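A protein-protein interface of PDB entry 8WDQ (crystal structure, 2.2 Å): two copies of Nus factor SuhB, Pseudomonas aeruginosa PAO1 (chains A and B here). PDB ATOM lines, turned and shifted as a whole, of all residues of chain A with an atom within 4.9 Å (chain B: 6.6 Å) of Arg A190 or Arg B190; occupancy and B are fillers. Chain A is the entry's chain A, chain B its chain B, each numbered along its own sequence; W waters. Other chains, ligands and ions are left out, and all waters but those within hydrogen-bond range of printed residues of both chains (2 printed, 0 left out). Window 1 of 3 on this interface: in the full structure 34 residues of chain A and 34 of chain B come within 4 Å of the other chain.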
ATOM      1  N   THR A 159      -3.348  25.138 -31.761  1.00  0.00           N
ATOM      2  CA  THR A 159      -2.361  25.828 -30.943  1.00  0.00           C
ATOM      3  C   THR A 159      -1.193  24.895 -30.665  1.00  0.00           C
ATOM      4  O   THR A 159      -1.242  23.698 -30.956  1.00  0.00           O
ATOM      5  CB  THR A 159      -2.980  26.337 -29.631  1.00  0.00           C
ATOM      6  OG1 THR A 159      -2.084  27.270 -29.007  1.00  0.00           O
ATOM      7  CG2 THR A 159      -3.259  25.174 -28.683  1.00  0.00           C
ATOM      8  N   GLY A 160      -0.137  25.470 -30.113  1.00  0.00           N
ATOM      9  CA  GLY A 160       0.991  24.692 -29.624  1.00  0.00           C
ATOM     10  C   GLY A 160       1.357  25.128 -28.222  1.00  0.00           C
ATOM     11  O   GLY A 160       1.324  26.318 -27.900  1.00  0.00           O
ATOM     12  N   PHE A 161       1.712  24.148 -27.388  1.00  0.00           N
ATOM     13  CA  PHE A 161       1.926  24.386 -25.965  1.00  0.00           C
ATOM     14  C   PHE A 161       3.359  24.846 -25.707  1.00  0.00           C
ATOM     15  O   PHE A 161       4.298  24.328 -26.317  1.00  0.00           O
ATOM     16  CB  PHE A 161       1.652  23.118 -25.153  1.00  0.00           C
ATOM     17  CG  PHE A 161       0.227  22.656 -25.203  1.00  0.00           C
ATOM     18  CD1 PHE A 161      -0.807  23.561 -25.414  1.00  0.00           C
ATOM     19  CD2 PHE A 161      -0.080  21.310 -25.036  1.00  0.00           C
ATOM     20  CE1 PHE A 161      -2.121  23.135 -25.452  1.00  0.00           C
ATOM     21  CE2 PHE A 161      -1.399  20.875 -25.073  1.00  0.00           C
ATOM     22  CZ  PHE A 161      -2.418  21.790 -25.274  1.00  0.00           C
ATOM     23  N   PHE A 163       6.103  24.141 -24.039  1.00  0.00           N
ATOM     24  CA  PHE A 163       6.535  22.972 -23.282  1.00  0.00           C
ATOM     25  C   PHE A 163       7.997  23.016 -22.856  1.00  0.00           C
ATOM     26  O   PHE A 163       8.393  22.227 -21.993  1.00  0.00           O
ATOM     27  CB  PHE A 163       6.291  21.698 -24.102  1.00  0.00           C
ATOM     28  CG  PHE A 163       7.109  21.625 -25.365  1.00  0.00           C
ATOM     29  CD1 PHE A 163       6.684  22.262 -26.520  1.00  0.00           C
ATOM     30  CD2 PHE A 163       8.302  20.917 -25.395  1.00  0.00           C
ATOM     31  CE1 PHE A 163       7.437  22.200 -27.684  1.00  0.00           C
ATOM     32  CE2 PHE A 163       9.060  20.845 -26.554  1.00  0.00           C
ATOM     33  CZ  PHE A 163       8.625  21.490 -27.700  1.00  0.00           C
ATOM     34  N   ILE A 188     -10.381  23.628 -29.017  1.00  0.00           N
ATOM     35  CA  ILE A 188      -8.975  23.952 -29.204  1.00  0.00           C
ATOM     36  C   ILE A 188      -8.234  22.634 -29.343  1.00  0.00           C
ATOM     37  O   ILE A 188      -8.513  21.682 -28.604  1.00  0.00           O
ATOM     38  CB  ILE A 188      -8.415  24.789 -28.038  1.00  0.00           C
ATOM     39  CG1 ILE A 188      -9.290  26.031 -27.820  1.00  0.00           C
ATOM     40  CG2 ILE A 188      -6.975  25.197 -28.320  1.00  0.00           C
ATOM     41  CD1 ILE A 188      -8.750  27.011 -26.807  1.00  0.00           C
ATOM     42  N   ARG A 189      -7.328  22.563 -30.315  1.00  0.00           N
ATOM     43  CA  ARG A 189      -6.643  21.327 -30.648  1.00  0.00           C
ATOM     44  C   ARG A 189      -5.140  21.554 -30.609  1.00  0.00           C
ATOM     45  O   ARG A 189      -4.631  22.551 -31.140  1.00  0.00           O
ATOM     46  CB  ARG A 189      -7.061  20.805 -32.037  1.00  0.00           C
ATOM     47  CG  ARG A 189      -8.556  20.546 -32.203  1.00  0.00           C
ATOM     48  CD  ARG A 189      -9.010  19.342 -31.384  1.00  0.00           C
ATOM     49  NE  ARG A 189     -10.449  19.107 -31.467  1.00  0.00           N
ATOM     50  CZ  ARG A 189     -11.328  19.506 -30.557  1.00  0.00           C
ATOM     51  NH1 ARG A 189     -10.958  20.214 -29.501  1.00  0.00           N
ATOM     52  NH2 ARG A 189     -12.609  19.182 -30.707  1.00  0.00           N
ATOM     53  N   ARG A 190      -4.433  20.612 -29.984  1.00  0.00           N
ATOM     54  CA  ARG A 190      -2.970  20.599 -29.953  1.00  0.00           C
ATOM     55  C   ARG A 190      -2.563  19.213 -30.436  1.00  0.00           C
ATOM     56  O   ARG A 190      -2.410  18.282 -29.638  1.00  0.00           O
ATOM     57  CB  ARG A 190      -2.428  20.913 -28.563  1.00  0.00           C
ATOM     58  CG  ARG A 190      -0.974  21.389 -28.553  1.00  0.00           C
ATOM     59  CD  ARG A 190       0.009  20.219 -28.569  1.00  0.00           C
ATOM     60  NE  ARG A 190       1.375  20.626 -28.253  1.00  0.00           N
ATOM     61  CZ  ARG A 190       2.217  21.188 -29.113  1.00  0.00           C
ATOM     62  NH1 ARG A 190       1.859  21.453 -30.359  1.00  0.00           N
ATOM     63  NH2 ARG A 190       3.453  21.485 -28.715  1.00  0.00           N
ATOM     64  N   ALA A 191      -2.410  19.075 -31.750  1.00  0.00           N
ATOM     65  CA  ALA A 191      -2.108  17.781 -32.340  1.00  0.00           C
ATOM     66  C   ALA A 191      -0.615  17.498 -32.419  1.00  0.00           C
ATOM     67  O   ALA A 191      -0.232  16.333 -32.584  1.00  0.00           O
ATOM     68  CB  ALA A 191      -2.729  17.682 -33.738  1.00  0.00           C
ATOM     69  N   GLY A 192       0.226  18.523 -32.319  1.00  0.00           N
ATOM     70  CA  GLY A 192       1.655  18.334 -32.168  1.00  0.00           C
ATOM     71  C   GLY A 192       2.516  18.493 -33.405  1.00  0.00           C
ATOM     72  O   GLY A 192       3.647  17.991 -33.407  1.00  0.00           O
ATOM     73  N   ALA A 193       2.038  19.175 -34.447  1.00  0.00           N
ATOM     74  CA  ALA A 193       2.877  19.445 -35.619  1.00  0.00           C
ATOM     75  C   ALA A 193       2.461  20.797 -36.191  1.00  0.00           C
ATOM     76  O   ALA A 193       1.433  20.897 -36.864  1.00  0.00           O
ATOM     77  CB  ALA A 193       2.760  18.334 -36.656  1.00  0.00           C
ATOM     78  N   GLU A 211       0.897  30.404 -31.591  1.00  0.00           N
ATOM     79  CA  GLU A 211       1.957  29.698 -30.872  1.00  0.00           C
ATOM     80  C   GLU A 211       3.178  30.596 -30.797  1.00  0.00           C
ATOM     81  O   GLU A 211       3.439  31.361 -31.720  1.00  0.00           O
ATOM     82  CB  GLU A 211       2.330  28.368 -31.558  1.00  0.00           C
ATOM     83  CG  GLU A 211       3.432  27.587 -30.837  1.00  0.00           C
ATOM     84  CD  GLU A 211       3.586  26.150 -31.328  1.00  0.00           C
ATOM     85  OE1 GLU A 211       2.940  25.773 -32.332  1.00  0.00           O
ATOM     86  OE2 GLU A 211       4.351  25.387 -30.695  1.00  0.00           O
ATOM     87  N   LEU B 157       1.527  12.771 -22.990  1.00  0.00           N
ATOM     88  CA  LEU B 157       0.202  12.563 -22.429  1.00  0.00           C
ATOM     89  C   LEU B 157      -0.874  12.974 -23.422  1.00  0.00           C
ATOM     90  O   LEU B 157      -0.695  13.899 -24.216  1.00  0.00           O
ATOM     91  CB  LEU B 157       0.024  13.354 -21.131  1.00  0.00           C
ATOM     92  CG  LEU B 157       1.110  13.186 -20.074  1.00  0.00           C
ATOM     93  CD1 LEU B 157       0.643  13.806 -18.776  1.00  0.00           C
ATOM     94  CD2 LEU B 157       1.456  11.707 -19.888  1.00  0.00           C
ATOM     95  N   GLY B 158      -1.997  12.265 -23.379  1.00  0.00           N
ATOM     96  CA  GLY B 158      -3.198  12.700 -24.050  1.00  0.00           C
ATOM     97  C   GLY B 158      -4.129  13.356 -23.053  1.00  0.00           C
ATOM     98  O   GLY B 158      -4.058  13.101 -21.855  1.00  0.00           O
ATOM     99  N   THR B 159      -5.000  14.223 -23.551  1.00  0.00           N
ATOM    100  CA  THR B 159      -5.979  14.839 -22.667  1.00  0.00           C
ATOM    101  C   THR B 159      -7.133  15.378 -23.498  1.00  0.00           C
ATOM    102  O   THR B 159      -7.061  15.456 -24.728  1.00  0.00           O
ATOM    103  CB  THR B 159      -5.344  15.950 -21.823  1.00  0.00           C
ATOM    104  OG1 THR B 159      -6.247  16.342 -20.775  1.00  0.00           O
ATOM    105  CG2 THR B 159      -5.003  17.153 -22.697  1.00  0.00           C
ATOM    106  N   GLY B 160      -8.211  15.732 -22.801  1.00  0.00           N
ATOM    107  CA  GLY B 160      -9.333  16.433 -23.393  1.00  0.00           C
ATOM    108  C   GLY B 160      -9.631  17.697 -22.613  1.00  0.00           C
ATOM    109  O   GLY B 160      -9.743  17.656 -21.383  1.00  0.00           O
ATOM    110  N   PHE B 161      -9.732  18.828 -23.309  1.00  0.00           N
ATOM    111  CA  PHE B 161      -9.992  20.095 -22.646  1.00  0.00           C
ATOM    112  C   PHE B 161     -11.437  20.151 -22.157  1.00  0.00           C
ATOM    113  O   PHE B 161     -12.344  19.630 -22.815  1.00  0.00           O
ATOM    114  CB  PHE B 161      -9.742  21.268 -23.592  1.00  0.00           C
ATOM    115  CG  PHE B 161      -8.339  21.355 -24.107  1.00  0.00           C
ATOM    116  CD1 PHE B 161      -7.267  21.010 -23.301  1.00  0.00           C
ATOM    117  CD2 PHE B 161      -8.093  21.785 -25.404  1.00  0.00           C
ATOM    118  CE1 PHE B 161      -5.975  21.095 -23.772  1.00  0.00           C
ATOM    119  CE2 PHE B 161      -6.802  21.875 -25.882  1.00  0.00           C
ATOM    120  CZ  PHE B 161      -5.741  21.531 -25.063  1.00  0.00           C
ATOM    121  N   PRO B 162     -11.682  20.800 -21.010  1.00  0.00           N
ATOM    122  CA  PRO B 162     -13.065  20.988 -20.512  1.00  0.00           C
ATOM    123  C   PRO B 162     -13.741  22.181 -21.184  1.00  0.00           C
ATOM    124  O   PRO B 162     -13.813  23.295 -20.659  1.00  0.00           O
ATOM    125  CB  PRO B 162     -12.854  21.202 -19.013  1.00  0.00           C
ATOM    126  CG  PRO B 162     -11.477  21.820 -18.901  1.00  0.00           C
ATOM    127  CD  PRO B 162     -10.679  21.416 -20.122  1.00  0.00           C
ATOM    128  N   PHE B 163     -14.266  21.925 -22.386  1.00  0.00           N
ATOM    129  CA  PHE B 163     -14.757  22.961 -23.287  1.00  0.00           C
ATOM    130  C   PHE B 163     -16.221  23.325 -23.070  1.00  0.00           C
ATOM    131  O   PHE B 163     -16.660  24.363 -23.579  1.00  0.00           O
ATOM    132  CB  PHE B 163     -14.557  22.525 -24.750  1.00  0.00           C
ATOM    133  CG  PHE B 163     -15.358  21.306 -25.138  1.00  0.00           C
ATOM    134  CD1 PHE B 163     -14.877  20.030 -24.885  1.00  0.00           C
ATOM    135  CD2 PHE B 163     -16.592  21.438 -25.755  1.00  0.00           C
ATOM    136  CE1 PHE B 163     -15.619  18.909 -25.237  1.00  0.00           C
ATOM    137  CE2 PHE B 163     -17.335  20.322 -26.109  1.00  0.00           C
ATOM    138  CZ  PHE B 163     -16.848  19.057 -25.849  1.00  0.00           C
ATOM    139  N   ARG B 164     -16.985  22.512 -22.342  1.00  0.00           N
ATOM    140  CA  ARG B 164     -18.415  22.760 -22.184  1.00  0.00           C
ATOM    141  C   ARG B 164     -18.677  23.893 -21.198  1.00  0.00           C
ATOM    142  O   ARG B 164     -17.877  24.158 -20.295  1.00  0.00           O
ATOM    143  CB  ARG B 164     -19.138  21.502 -21.696  1.00  0.00           C
ATOM    144  CG  ARG B 164     -19.084  20.317 -22.639  1.00  0.00           C
ATOM    145  CD  ARG B 164     -19.481  19.040 -21.909  1.00  0.00           C
ATOM    146  NE  ARG B 164     -19.216  17.850 -22.706  1.00  0.00           N
ATOM    147  CZ  ARG B 164     -18.034  17.256 -22.789  1.00  0.00           C
ATOM    148  NH1 ARG B 164     -16.985  17.707 -22.119  1.00  0.00           N
ATOM    149  NH2 ARG B 164     -17.899  16.183 -23.564  1.00  0.00           N
ATOM    150  N   TYR B 174      -8.597  22.337 -14.015  1.00  0.00           N
ATOM    151  CA  TYR B 174      -7.948  21.649 -15.120  1.00  0.00           C
ATOM    152  C   TYR B 174      -6.640  22.335 -15.484  1.00  0.00           C
ATOM    153  O   TYR B 174      -5.593  21.684 -15.593  1.00  0.00           O
ATOM    154  CB  TYR B 174      -8.872  21.594 -16.333  1.00  0.00           C
ATOM    155  CG  TYR B 174      -8.226  20.874 -17.483  1.00  0.00           C
ATOM    156  CD1 TYR B 174      -8.206  19.486 -17.533  1.00  0.00           C
ATOM    157  CD2 TYR B 174      -7.577  21.579 -18.485  1.00  0.00           C
ATOM    158  CE1 TYR B 174      -7.598  18.822 -18.580  1.00  0.00           C
ATOM    159  CE2 TYR B 174      -6.958  20.929 -19.530  1.00  0.00           C
ATOM    160  CZ  TYR B 174      -6.970  19.552 -19.571  1.00  0.00           C
ATOM    161  OH  TYR B 174      -6.354  18.906 -20.606  1.00  0.00           O
ATOM    162  N   GLY B 187       5.448  16.234 -23.787  1.00  0.00           N
ATOM    163  CA  GLY B 187       4.374  16.900 -24.485  1.00  0.00           C
ATOM    164  C   GLY B 187       3.026  16.455 -23.965  1.00  0.00           C
ATOM    165  O   GLY B 187       2.881  15.383 -23.364  1.00  0.00           O
ATOM    166  N   ILE B 188       2.041  17.314 -24.205  1.00  0.00           N
ATOM    167  CA  ILE B 188       0.635  17.028 -23.970  1.00  0.00           C
ATOM    168  C   ILE B 188      -0.093  17.253 -25.289  1.00  0.00           C
ATOM    169  O   ILE B 188       0.195  18.222 -26.000  1.00  0.00           O
ATOM    170  CB  ILE B 188       0.052  17.918 -22.852  1.00  0.00           C
ATOM    171  CG1 ILE B 188       0.940  17.860 -21.603  1.00  0.00           C
ATOM    172  CG2 ILE B 188      -1.380  17.508 -22.529  1.00  0.00           C
ATOM    173  CD1 ILE B 188       0.489  18.770 -20.472  1.00  0.00           C
ATOM    174  N   ARG B 189      -1.019  16.354 -25.619  1.00  0.00           N
ATOM    175  CA  ARG B 189      -1.730  16.390 -26.888  1.00  0.00           C
ATOM    176  C   ARG B 189      -3.231  16.381 -26.649  1.00  0.00           C
ATOM    177  O   ARG B 189      -3.740  15.601 -25.833  1.00  0.00           O
ATOM    178  CB  ARG B 189      -1.344  15.203 -27.780  1.00  0.00           C
ATOM    179  CG  ARG B 189       0.141  15.128 -28.121  1.00  0.00           C
ATOM    180  CD  ARG B 189       0.531  16.209 -29.125  1.00  0.00           C
ATOM    181  NE  ARG B 189       1.953  16.161 -29.445  1.00  0.00           N
ATOM    182  CZ  ARG B 189       2.889  16.827 -28.784  1.00  0.00           C
ATOM    183  NH1 ARG B 189       2.582  17.633 -27.779  1.00  0.00           N
ATOM    184  NH2 ARG B 189       4.164  16.680 -29.137  1.00  0.00           N
ATOM    185  N   ARG B 190      -3.938  17.241 -27.384  1.00  0.00           N
ATOM    186  CA  ARG B 190      -5.401  17.276 -27.389  1.00  0.00           C
ATOM    187  C   ARG B 190      -5.832  17.210 -28.853  1.00  0.00           C
ATOM    188  O   ARG B 190      -5.972  18.242 -29.518  1.00  0.00           O
ATOM    189  CB  ARG B 190      -5.935  18.519 -26.676  1.00  0.00           C
ATOM    190  CG  ARG B 190      -7.381  18.388 -26.188  1.00  0.00           C
ATOM    191  CD  ARG B 190      -8.392  18.650 -27.311  1.00  0.00           C
ATOM    192  NE  ARG B 190      -9.757  18.847 -26.831  1.00  0.00           N
ATOM    193  CZ  ARG B 190     -10.619  17.868 -26.587  1.00  0.00           C
ATOM    194  NH1 ARG B 190     -10.287  16.596 -26.747  1.00  0.00           N
ATOM    195  NH2 ARG B 190     -11.847  18.173 -26.171  1.00  0.00           N
ATOM    196  N   ALA B 191      -6.045  15.989 -29.350  1.00  0.00           N
ATOM    197  CA  ALA B 191      -6.337  15.769 -30.761  1.00  0.00           C
ATOM    198  C   ALA B 191      -7.828  15.728 -31.081  1.00  0.00           C
ATOM    199  O   ALA B 191      -8.196  15.903 -32.249  1.00  0.00           O
ATOM    200  CB  ALA B 191      -5.675  14.475 -31.236  1.00  0.00           C
ATOM    201  N   GLY B 192      -8.685  15.477 -30.097  1.00  0.00           N
ATOM    202  CA  GLY B 192     -10.117  15.660 -30.267  1.00  0.00           C
ATOM    203  C   GLY B 192     -10.982  14.421 -30.438  1.00  0.00           C
ATOM    204  O   GLY B 192     -12.101  14.546 -30.948  1.00  0.00           O
ATOM    205  N   ALA B 193     -10.528  13.243 -30.016  1.00  0.00           N
ATOM    206  CA  ALA B 193     -11.405  12.071 -30.010  1.00  0.00           C
ATOM    207  C   ALA B 193     -10.951  11.157 -28.880  1.00  0.00           C
ATOM    208  O   ALA B 193      -9.875  10.558 -28.964  1.00  0.00           O
ATOM    209  CB  ALA B 193     -11.390  11.349 -31.357  1.00  0.00           C
ATOM    210  N   ALA B 194     -11.767  11.053 -27.828  1.00  0.00           N
ATOM    211  CA  ALA B 194     -11.327  10.375 -26.608  1.00  0.00           C
ATOM    212  C   ALA B 194     -11.136   8.883 -26.834  1.00  0.00           C
ATOM    213  O   ALA B 194     -10.263   8.262 -26.215  1.00  0.00           O
ATOM    214  CB  ALA B 194     -12.326  10.611 -25.475  1.00  0.00           C
ATOM    215  N   ASP B 197      -7.765   8.618 -28.100  1.00  0.00           N
ATOM    216  CA  ASP B 197      -6.794   8.863 -27.032  1.00  0.00           C
ATOM    217  C   ASP B 197      -6.584   7.611 -26.189  1.00  0.00           C
ATOM    218  O   ASP B 197      -5.444   7.245 -25.857  1.00  0.00           O
ATOM    219  CB  ASP B 197      -7.254  10.025 -26.147  1.00  0.00           C
ATOM    220  CG  ASP B 197      -7.261  11.360 -26.882  1.00  0.00           C
ATOM    221  OD1 ASP B 197      -6.345  11.599 -27.698  1.00  0.00           O
ATOM    222  OD2 ASP B 197      -8.183  12.173 -26.639  1.00  0.00           O
ATOM    223  N   TYR B 206       0.506   7.054 -26.409  1.00  0.00           N
ATOM    224  CA  TYR B 206       0.483   7.934 -25.250  1.00  0.00           C
ATOM    225  C   TYR B 206       0.867   7.125 -24.020  1.00  0.00           C
ATOM    226  O   TYR B 206       0.547   5.937 -23.914  1.00  0.00           O
ATOM    227  CB  TYR B 206      -0.893   8.559 -25.016  1.00  0.00           C
ATOM    228  CG  TYR B 206      -1.353   9.553 -26.060  1.00  0.00           C
ATOM    229  CD1 TYR B 206      -0.450  10.178 -26.911  1.00  0.00           C
ATOM    230  CD2 TYR B 206      -2.699   9.866 -26.185  1.00  0.00           C
ATOM    231  CE1 TYR B 206      -0.882  11.092 -27.861  1.00  0.00           C
ATOM    232  CE2 TYR B 206      -3.142  10.769 -27.126  1.00  0.00           C
ATOM    233  CZ  TYR B 206      -2.236  11.380 -27.964  1.00  0.00           C
ATOM    234  OH  TYR B 206      -2.704  12.281 -28.898  1.00  0.00           O
ATOM    235  N   PHE B 209      -3.365   9.438 -20.079  1.00  0.00           N
ATOM    236  CA  PHE B 209      -4.467  10.248 -20.573  1.00  0.00           C
ATOM    237  C   PHE B 209      -5.400  10.521 -19.404  1.00  0.00           C
ATOM    238  O   PHE B 209      -5.608   9.645 -18.561  1.00  0.00           O
ATOM    239  CB  PHE B 209      -5.220   9.524 -21.701  1.00  0.00           C
ATOM    240  CG  PHE B 209      -6.576  10.113 -22.025  1.00  0.00           C
ATOM    241  CD1 PHE B 209      -6.693  11.196 -22.883  1.00  0.00           C
ATOM    242  CD2 PHE B 209      -7.734   9.563 -21.496  1.00  0.00           C
ATOM    243  CE1 PHE B 209      -7.946  11.732 -23.192  1.00  0.00           C
ATOM    244  CE2 PHE B 209      -8.978  10.083 -21.804  1.00  0.00           C
ATOM    245  CZ  PHE B 209      -9.084  11.176 -22.656  1.00  0.00           C
ATOM    246  N   GLU B 211      -9.222  12.930 -18.544  1.00  0.00           N
ATOM    247  CA  GLU B 211     -10.278  13.823 -19.011  1.00  0.00           C
ATOM    248  C   GLU B 211     -11.488  13.655 -18.101  1.00  0.00           C
ATOM    249  O   GLU B 211     -11.698  12.582 -17.534  1.00  0.00           O
ATOM    250  CB  GLU B 211     -10.658  13.528 -20.477  1.00  0.00           C
ATOM    251  CG  GLU B 211     -11.832  14.357 -21.004  1.00  0.00           C
ATOM    252  CD  GLU B 211     -11.958  14.352 -22.518  1.00  0.00           C
ATOM    253  OE1 GLU B 211     -11.333  13.500 -23.184  1.00  0.00           O
ATOM    254  OE2 GLU B 211     -12.692  15.214 -23.045  1.00  0.00           O
HETATM  255  O   HOH W   1     -13.494  16.663 -32.264  1.00  0.00           O
HETATM  256  O   HOH W   2       5.140  16.284 -31.799  1.00  0.00           O
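Water W2 bridges the backbone carbonyl oxygen (O) of Gly A192 (2.8 Å) and the guanidinium group (NH2) of Arg B189 (2.9 Å).
Water W1 bridges the backbone carbonyl oxygen (O) of Gly B192 (2.9 Å) and the guanidinium group (NH2) of Arg A189 (3.1 Å).
Of the printed residues of chain B, Phe A161 touches Phe B161 and Ile B188.
Of chain B, only Ile B188, Arg B189 and Arg B190 come within 4 Å of Arg A190.
Of the printed residues of chain B, Gly A192 touches Arg B189.
Printed residues of chain A within 4 Å of Arg B189: Arg A190 (3.3 Å), Ala A191 (3.5 Å) and Gly A192 (3.5 Å).
Of chain A, only Ile A188 (3.3 Å), Arg A189 (3.2 Å) and Arg A190 (2.9 Å) come within 4 Å of Arg B190.
Glu B211 touches none of the printed residues of chain A.
The nearest residue of chain B that does not touch Arg A190 is Ala B191 (4.3 Å).
O of Arg B189 sits at hydrogen-bond distance from N of Thr B159, 2.9 Å away.
O of Arg A189 sits at hydrogen-bond distance from N of Thr A159.
N of Arg B189 lies within hydrogen-bond range of O of Leu B157.
Ile A188 touches Arg B190, and with the chains exchanged Arg A190 touches Ile B188.
Arg A189 touches Ala B191, and with the chains exchanged Ala A191 touches Arg B189.
Arg A189 touches Gly B192, and with the chains exchanged Gly A192 touches Arg B189.
Arg A190 touches its own counterpart, Arg B190.
Of the 21 printed residues of chain B, 6 touch a printed residue of chain A.
Hydrophobic or aromatic side chains of chain B that line the printed part of chain A: Phe B161 and Ile B188.
Of the 11 printed residues of chain A, 6 touch a printed residue of chain B.
Hydrophobic or aromatic side chains of chain A within 4 Å of the printed part of chain B: Phe A161 and Ile A188.
Among the printed residues, 12 pairs touch across the chains.
The guanidinium group (NH1) of Arg A189 lies close to the guanidinium group (NE) of Arg B190, at 3.2 Å.
The backbone carbonyl oxygen (O) of Ile B188 lies close to the guanidinium group (NE) of Arg A190, at 3.5 Å.
The backbone carbonyl oxygen (O) of Arg B190 sits at hydrogen-bond distance from the backbone NH (N) of Arg A190 (2.9 Å).
NE of Arg A190 sits close to NH1 of Arg B189 (3.3 Å).
Phe A161 touches Phe B161.
Phe A161 touches Ile B188.
Ile A188 touches Phe B161.
Ile A188 touches Arg B190 (O to CD, 3.3 Å).
O of Ala B191 touches CD of Arg A189, 3.6 Å away.
Gly B192 touches Arg A189 (CA to NE, 3.7 Å).
Ala A191 touches Arg B189.
CA of Gly A192 touches NE of Arg B189 (3.5 Å).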
